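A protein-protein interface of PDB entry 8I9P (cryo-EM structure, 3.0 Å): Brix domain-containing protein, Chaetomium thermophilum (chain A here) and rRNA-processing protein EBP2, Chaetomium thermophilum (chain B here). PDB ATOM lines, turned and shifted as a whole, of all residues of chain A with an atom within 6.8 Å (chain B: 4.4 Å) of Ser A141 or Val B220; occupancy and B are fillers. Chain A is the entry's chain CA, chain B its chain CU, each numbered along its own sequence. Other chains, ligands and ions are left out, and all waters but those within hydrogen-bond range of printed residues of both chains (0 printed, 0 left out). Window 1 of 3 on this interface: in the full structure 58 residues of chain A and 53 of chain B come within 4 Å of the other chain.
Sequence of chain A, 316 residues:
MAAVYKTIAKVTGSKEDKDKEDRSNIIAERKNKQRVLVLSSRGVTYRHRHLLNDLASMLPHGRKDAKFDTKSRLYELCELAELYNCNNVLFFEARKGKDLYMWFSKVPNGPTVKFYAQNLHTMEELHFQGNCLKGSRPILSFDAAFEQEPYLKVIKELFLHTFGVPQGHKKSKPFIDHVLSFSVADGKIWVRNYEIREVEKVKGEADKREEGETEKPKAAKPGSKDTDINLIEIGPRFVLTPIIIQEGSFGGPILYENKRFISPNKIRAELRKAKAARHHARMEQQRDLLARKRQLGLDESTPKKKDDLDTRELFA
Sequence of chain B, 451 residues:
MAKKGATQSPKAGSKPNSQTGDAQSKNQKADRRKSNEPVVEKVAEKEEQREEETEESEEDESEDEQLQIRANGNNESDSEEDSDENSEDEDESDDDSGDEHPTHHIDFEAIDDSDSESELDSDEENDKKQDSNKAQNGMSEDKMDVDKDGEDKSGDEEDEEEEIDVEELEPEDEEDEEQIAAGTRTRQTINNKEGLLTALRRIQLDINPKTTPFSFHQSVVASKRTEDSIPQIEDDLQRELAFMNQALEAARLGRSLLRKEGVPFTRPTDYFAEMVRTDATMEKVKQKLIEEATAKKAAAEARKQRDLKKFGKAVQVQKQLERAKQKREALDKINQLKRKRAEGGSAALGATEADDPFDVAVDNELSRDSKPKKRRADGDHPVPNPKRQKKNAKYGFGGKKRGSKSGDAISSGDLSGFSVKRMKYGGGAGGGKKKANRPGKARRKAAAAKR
Among the printed residues, pairs that only touch across the chains: Pro A138 with Gln B218, Ile A139 with Gln B218, Ile A139 with Val B220, Leu A140 with Ser B219, Ser A141 with Val B220, Ser A141 with Ala B250, Phe A142 with Ser B219, Phe A142 with Val B221, Phe A142 with Gln B246, Asp A143 with Val B221, Asp A143 with Gln B246 and Ser A183 with Gln B246.
NE2 of Gln B246 lies within hydrogen-bond range of OG of Ser A181 (3.3 Å). The backbone carbonyl oxygen (O) of Gln B218 is in hydrogen-bond range of the backbone NH (N) of Leu A140 (3.0 Å). The backbone NH (N) of Ala B222 lies within hydrogen-bond range of the backbone carbonyl oxygen (O) of Phe A142, at 3.4 Å. The side-chain amide nitrogen (NE2) of Gln B246 sits at hydrogen-bond distance from the backbone carbonyl oxygen (O) of Phe A182 (3.1 Å). The side-chain amide nitrogen (NE2) of Gln B246 lies within hydrogen-bond range of the side-chain hydroxyl (OG) of Ser A141 (2.8 Å). The backbone NH of Val B220 sits at hydrogen-bond distance from the backbone carbonyl oxygen of Leu A140 (3.3 Å). O of Val B220 is in hydrogen-bond range of N of Phe A142 (3.3 Å).
Of the 13 printed residues of chain A, 9 touch a printed residue of chain B. Among the printed residues, no Asp or Glu carboxylate lies within 4 Å of a Lys or Arg side-chain nitrogen of the other chain.
OG of Ser A141 sits close to OG of Ser A181 (3.2 Å). The backbone carbonyl oxygen (O) of Leu A180 lies within hydrogen-bond range of the backbone NH (N) of Ser A141 (3.0 Å). The backbone NH (N) of Phe A182 is in hydrogen-bond range of the backbone carbonyl oxygen (O) of Ser A141. The backbone carbonyl oxygen of Ile A139 is in hydrogen-bond range of the backbone NH of Leu A180 (3.0 Å).
Ser A141 touches three residues of chain B. Of chain A, only Ile A139, Leu A140, Ser A141 and Phe A142 come within 4 Å of Val B220. Printed residues of chain A within 4 Å of Gln B218: Pro A138, Ile A139 and Leu A140. Printed residues of chain B within 4 Å of Leu A140: Gln B218 (3.0 Å), Ser B219 (3.7 Å) and Val B220 (3.2 Å). Val A179 touches none of the printed residues of chain B. Tyr A194 touches none of the printed residues of chain B. The nearest printed residue of chain B that does not touch Ser A141 is Val B221 (5.6 Å). The nearest printed residue of chain A that does not touch Gln B246 is Leu A180 (6.0 Å).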
ATOM      1  N   PRO A 138     -30.455  18.614  35.247  1.00  0.00           N
ATOM      2  CA  PRO A 138     -29.818  18.845  33.950  1.00  0.00           C
ATOM      3  C   PRO A 138     -28.945  17.678  33.543  1.00  0.00           C
ATOM      4  O   PRO A 138     -28.440  16.933  34.389  1.00  0.00           O
ATOM      5  CB  PRO A 138     -28.994  20.113  34.192  1.00  0.00           C
ATOM      6  CG  PRO A 138     -28.656  20.054  35.658  1.00  0.00           C
ATOM      7  CD  PRO A 138     -29.666  19.178  36.356  1.00  0.00           C
ATOM      8  N   ILE A 139     -28.779  17.489  32.246  1.00  0.00           N
ATOM      9  CA  ILE A 139     -27.803  16.526  31.770  1.00  0.00           C
ATOM     10  C   ILE A 139     -26.443  17.204  31.810  1.00  0.00           C
ATOM     11  O   ILE A 139     -26.222  18.217  31.138  1.00  0.00           O
ATOM     12  CB  ILE A 139     -28.158  16.040  30.359  1.00  0.00           C
ATOM     13  CG1 ILE A 139     -29.626  15.618  30.311  1.00  0.00           C
ATOM     14  CG2 ILE A 139     -27.293  14.865  29.984  1.00  0.00           C
ATOM     15  CD1 ILE A 139     -30.449  16.395  29.310  1.00  0.00           C
ATOM     16  N   LEU A 140     -25.545  16.679  32.633  1.00  0.00           N
ATOM     17  CA  LEU A 140     -24.229  17.284  32.806  1.00  0.00           C
ATOM     18  C   LEU A 140     -23.320  16.701  31.734  1.00  0.00           C
ATOM     19  O   LEU A 140     -22.915  15.540  31.808  1.00  0.00           O
ATOM     20  CB  LEU A 140     -23.698  17.042  34.214  1.00  0.00           C
ATOM     21  CG  LEU A 140     -24.436  17.732  35.370  1.00  0.00           C
ATOM     22  CD1 LEU A 140     -23.512  17.909  36.556  1.00  0.00           C
ATOM     23  CD2 LEU A 140     -25.022  19.078  34.960  1.00  0.00           C
ATOM     24  N   SER A 141     -23.014  17.513  30.725  1.00  0.00           N
ATOM     25  CA  SER A 141     -22.241  17.065  29.569  1.00  0.00           C
ATOM     26  C   SER A 141     -20.779  17.373  29.841  1.00  0.00           C
ATOM     27  O   SER A 141     -20.354  18.529  29.853  1.00  0.00           O
ATOM     28  CB  SER A 141     -22.718  17.748  28.298  1.00  0.00           C
ATOM     29  OG  SER A 141     -21.883  18.840  27.973  1.00  0.00           O
ATOM     30  N   PHE A 142     -19.999  16.326  30.070  1.00  0.00           N
ATOM     31  CA  PHE A 142     -18.573  16.493  30.296  1.00  0.00           C
ATOM     32  C   PHE A 142     -17.837  16.339  28.965  1.00  0.00           C
ATOM     33  O   PHE A 142     -18.424  16.019  27.929  1.00  0.00           O
ATOM     34  CB  PHE A 142     -18.089  15.506  31.354  1.00  0.00           C
ATOM     35  CG  PHE A 142     -18.611  15.796  32.733  1.00  0.00           C
ATOM     36  CD1 PHE A 142     -18.213  16.932  33.420  1.00  0.00           C
ATOM     37  CD2 PHE A 142     -19.504  14.930  33.343  1.00  0.00           C
ATOM     38  CE1 PHE A 142     -18.702  17.199  34.687  1.00  0.00           C
ATOM     39  CE2 PHE A 142     -19.992  15.190  34.609  1.00  0.00           C
ATOM     40  CZ  PHE A 142     -19.589  16.326  35.282  1.00  0.00           C
ATOM     41  N   ASP A 143     -16.530  16.586  28.989  1.00  0.00           N
ATOM     42  CA  ASP A 143     -15.615  16.460  27.874  1.00  0.00           C
ATOM     43  C   ASP A 143     -14.815  15.173  28.102  1.00  0.00           C
ATOM     44  O   ASP A 143     -14.724  14.699  29.248  1.00  0.00           O
ATOM     45  CB  ASP A 143     -14.780  17.745  27.794  1.00  0.00           C
ATOM     46  CG  ASP A 143     -13.612  17.691  26.788  1.00  0.00           C
ATOM     47  OD1 ASP A 143     -12.793  16.746  26.756  1.00  0.00           O
ATOM     48  OD2 ASP A 143     -13.507  18.658  26.008  1.00  0.00           O
ATOM     49  N   PHE A 146     -12.141  15.025  30.761  1.00  0.00           N
ATOM     50  CA  PHE A 146     -12.521  15.011  32.170  1.00  0.00           C
ATOM     51  C   PHE A 146     -12.290  13.654  32.823  1.00  0.00           C
ATOM     52  O   PHE A 146     -12.586  13.501  34.012  1.00  0.00           O
ATOM     53  CB  PHE A 146     -13.984  15.427  32.339  1.00  0.00           C
ATOM     54  CG  PHE A 146     -14.187  16.914  32.450  1.00  0.00           C
ATOM     55  CD1 PHE A 146     -13.561  17.638  33.447  1.00  0.00           C
ATOM     56  CD2 PHE A 146     -15.020  17.583  31.575  1.00  0.00           C
ATOM     57  CE1 PHE A 146     -13.750  19.002  33.559  1.00  0.00           C
ATOM     58  CE2 PHE A 146     -15.215  18.948  31.678  1.00  0.00           C
ATOM     59  CZ  PHE A 146     -14.577  19.657  32.672  1.00  0.00           C
ATOM     60  N   VAL A 179     -29.510  20.862  28.976  1.00  0.00           N
ATOM     61  CA  VAL A 179     -28.223  20.198  29.139  1.00  0.00           C
ATOM     62  C   VAL A 179     -27.166  21.272  29.368  1.00  0.00           C
ATOM     63  O   VAL A 179     -27.107  22.266  28.634  1.00  0.00           O
ATOM     64  CB  VAL A 179     -27.886  19.308  27.921  1.00  0.00           C
ATOM     65  CG1 VAL A 179     -28.139  20.042  26.608  1.00  0.00           C
ATOM     66  CG2 VAL A 179     -26.444  18.825  27.975  1.00  0.00           C
ATOM     67  N   LEU A 180     -26.359  21.097  30.408  1.00  0.00           N
ATOM     68  CA  LEU A 180     -25.347  22.081  30.766  1.00  0.00           C
ATOM     69  C   LEU A 180     -23.986  21.590  30.284  1.00  0.00           C
ATOM     70  O   LEU A 180     -23.555  20.488  30.637  1.00  0.00           O
ATOM     71  CB  LEU A 180     -25.363  22.334  32.273  1.00  0.00           C
ATOM     72  CG  LEU A 180     -24.521  23.496  32.791  1.00  0.00           C
ATOM     73  CD1 LEU A 180     -25.355  24.757  32.823  1.00  0.00           C
ATOM     74  CD2 LEU A 180     -24.046  23.172  34.186  1.00  0.00           C
ATOM     75  N   SER A 181     -23.319  22.410  29.477  1.00  0.00           N
ATOM     76  CA  SER A 181     -22.179  21.974  28.687  1.00  0.00           C
ATOM     77  C   SER A 181     -20.859  22.426  29.297  1.00  0.00           C
ATOM     78  O   SER A 181     -20.642  23.613  29.556  1.00  0.00           O
ATOM     79  CB  SER A 181     -22.288  22.499  27.255  1.00  0.00           C
ATOM     80  OG  SER A 181     -21.639  21.630  26.343  1.00  0.00           O
ATOM     81  N   PHE A 182     -19.975  21.449  29.507  1.00  0.00           N
ATOM     82  CA  PHE A 182     -18.609  21.657  29.995  1.00  0.00           C
ATOM     83  C   PHE A 182     -17.689  21.207  28.866  1.00  0.00           C
ATOM     84  O   PHE A 182     -17.770  20.054  28.431  1.00  0.00           O
ATOM     85  CB  PHE A 182     -18.346  20.843  31.257  1.00  0.00           C
ATOM     86  CG  PHE A 182     -19.190  21.234  32.435  1.00  0.00           C
ATOM     87  CD1 PHE A 182     -19.722  22.504  32.549  1.00  0.00           C
ATOM     88  CD2 PHE A 182     -19.480  20.301  33.417  1.00  0.00           C
ATOM     89  CE1 PHE A 182     -20.498  22.847  33.638  1.00  0.00           C
ATOM     90  CE2 PHE A 182     -20.264  20.632  34.500  1.00  0.00           C
ATOM     91  CZ  PHE A 182     -20.768  21.906  34.615  1.00  0.00           C
ATOM     92  N   SER A 183     -16.817  22.090  28.389  1.00  0.00           N
ATOM     93  CA  SER A 183     -15.909  21.737  27.305  1.00  0.00           C
ATOM     94  C   SER A 183     -14.529  22.340  27.532  1.00  0.00           C
ATOM     95  O   SER A 183     -14.409  23.526  27.837  1.00  0.00           O
ATOM     96  CB  SER A 183     -16.475  22.201  25.964  1.00  0.00           C
ATOM     97  OG  SER A 183     -17.121  23.454  26.097  1.00  0.00           O
ATOM     98  N   TYR A 194     -27.946  24.689  27.264  1.00  0.00           N
ATOM     99  CA  TYR A 194     -28.718  24.507  26.044  1.00  0.00           C
ATOM    100  C   TYR A 194     -30.081  23.916  26.376  1.00  0.00           C
ATOM    101  O   TYR A 194     -30.208  23.069  27.261  1.00  0.00           O
ATOM    102  CB  TYR A 194     -27.969  23.599  25.066  1.00  0.00           C
ATOM    103  CG  TYR A 194     -26.659  24.174  24.580  1.00  0.00           C
ATOM    104  CD1 TYR A 194     -26.618  25.368  23.872  1.00  0.00           C
ATOM    105  CD2 TYR A 194     -25.459  23.551  24.879  1.00  0.00           C
ATOM    106  CE1 TYR A 194     -25.416  25.891  23.429  1.00  0.00           C
ATOM    107  CE2 TYR A 194     -24.254  24.068  24.447  1.00  0.00           C
ATOM    108  CZ  TYR A 194     -24.238  25.240  23.728  1.00  0.00           C
ATOM    109  OH  TYR A 194     -23.039  25.761  23.301  1.00  0.00           O
ATOM    110  N   GLN B 218     -27.181  11.586  36.296  1.00  0.00           N
ATOM    111  CA  GLN B 218     -27.618  12.346  35.118  1.00  0.00           C
ATOM    112  C   GLN B 218     -26.419  12.943  34.383  1.00  0.00           C
ATOM    113  O   GLN B 218     -26.468  14.065  33.874  1.00  0.00           O
ATOM    114  CB  GLN B 218     -28.640  13.425  35.484  1.00  0.00           C
ATOM    115  CG  GLN B 218     -29.643  13.708  34.382  1.00  0.00           C
ATOM    116  CD  GLN B 218     -31.021  14.031  34.914  1.00  0.00           C
ATOM    117  OE1 GLN B 218     -31.461  13.472  35.918  1.00  0.00           O
ATOM    118  NE2 GLN B 218     -31.727  14.905  34.217  1.00  0.00           N
ATOM    119  N   SER B 219     -25.331  12.182  34.333  1.00  0.00           N
ATOM    120  CA  SER B 219     -24.068  12.633  33.773  1.00  0.00           C
ATOM    121  C   SER B 219     -23.644  11.706  32.646  1.00  0.00           C
ATOM    122  O   SER B 219     -23.567  10.486  32.826  1.00  0.00           O
ATOM    123  CB  SER B 219     -22.978  12.675  34.846  1.00  0.00           C
ATOM    124  OG  SER B 219     -22.559  11.365  35.190  1.00  0.00           O
ATOM    125  N   VAL B 220     -23.369  12.291  31.485  1.00  0.00           N
ATOM    126  CA  VAL B 220     -22.885  11.559  30.324  1.00  0.00           C
ATOM    127  C   VAL B 220     -21.641  12.274  29.806  1.00  0.00           C
ATOM    128  O   VAL B 220     -21.606  13.509  29.747  1.00  0.00           O
ATOM    129  CB  VAL B 220     -23.970  11.416  29.238  1.00  0.00           C
ATOM    130  CG1 VAL B 220     -24.525  12.760  28.819  1.00  0.00           C
ATOM    131  CG2 VAL B 220     -23.434  10.671  28.036  1.00  0.00           C
ATOM    132  N   VAL B 221     -20.602  11.505  29.500  1.00  0.00           N
ATOM    133  CA  VAL B 221     -19.327  12.060  29.069  1.00  0.00           C
ATOM    134  C   VAL B 221     -19.139  11.783  27.584  1.00  0.00           C
ATOM    135  O   VAL B 221     -19.327  10.650  27.124  1.00  0.00           O
ATOM    136  CB  VAL B 221     -18.170  11.475  29.892  1.00  0.00           C
ATOM    137  CG1 VAL B 221     -16.930  12.308  29.694  1.00  0.00           C
ATOM    138  CG2 VAL B 221     -18.546  11.412  31.366  1.00  0.00           C
ATOM    139  N   ALA B 222     -18.771  12.818  26.833  1.00  0.00           N
ATOM    140  CA  ALA B 222     -18.587  12.695  25.395  1.00  0.00           C
ATOM    141  C   ALA B 222     -17.344  11.876  25.070  1.00  0.00           C
ATOM    142  O   ALA B 222     -16.337  11.934  25.782  1.00  0.00           O
ATOM    143  CB  ALA B 222     -18.479  14.075  24.751  1.00  0.00           C
ATOM    144  N   GLN B 246     -21.080  18.475  20.971  1.00  0.00           N
ATOM    145  CA  GLN B 246     -20.895  17.757  22.233  1.00  0.00           C
ATOM    146  C   GLN B 246     -22.188  17.684  23.039  1.00  0.00           C
ATOM    147  O   GLN B 246     -22.564  16.604  23.524  1.00  0.00           O
ATOM    148  CB  GLN B 246     -19.799  18.424  23.066  1.00  0.00           C
ATOM    149  CG  GLN B 246     -19.391  17.627  24.293  1.00  0.00           C
ATOM    150  CD  GLN B 246     -18.821  18.493  25.399  1.00  0.00           C
ATOM    151  OE1 GLN B 246     -17.625  18.784  25.423  1.00  0.00           O
ATOM    152  NE2 GLN B 246     -19.679  18.916  26.320  1.00  0.00           N
ATOM    153  N   ALA B 250     -24.621  14.483  24.047  1.00  0.00           N
ATOM    154  CA  ALA B 250     -25.080  14.281  25.417  1.00  0.00           C
ATOM    155  C   ALA B 250     -26.600  14.194  25.497  1.00  0.00           C
ATOM    156  O   ALA B 250     -27.138  13.336  26.204  1.00  0.00           O
ATOM    157  CB  ALA B 250     -24.570  15.413  26.300  1.00  0.00           C
ATOM    158  N   LEU B 253     -27.867  10.794  24.003  1.00  0.00           N
ATOM    159  CA  LEU B 253     -27.618   9.617  24.832  1.00  0.00           C
ATOM    160  C   LEU B 253     -28.422   9.684  26.130  1.00  0.00           C
ATOM    161  O   LEU B 253     -28.932   8.659  26.605  1.00  0.00           O
ATOM    162  CB  LEU B 253     -26.111   9.473  25.078  1.00  0.00           C
ATOM    163  CG  LEU B 253     -25.460   8.097  25.327  1.00  0.00           C
ATOM    164  CD1 LEU B 253     -23.949   8.237  25.367  1.00  0.00           C
ATOM    165  CD2 LEU B 253     -25.924   7.400  26.598  1.00  0.00           C
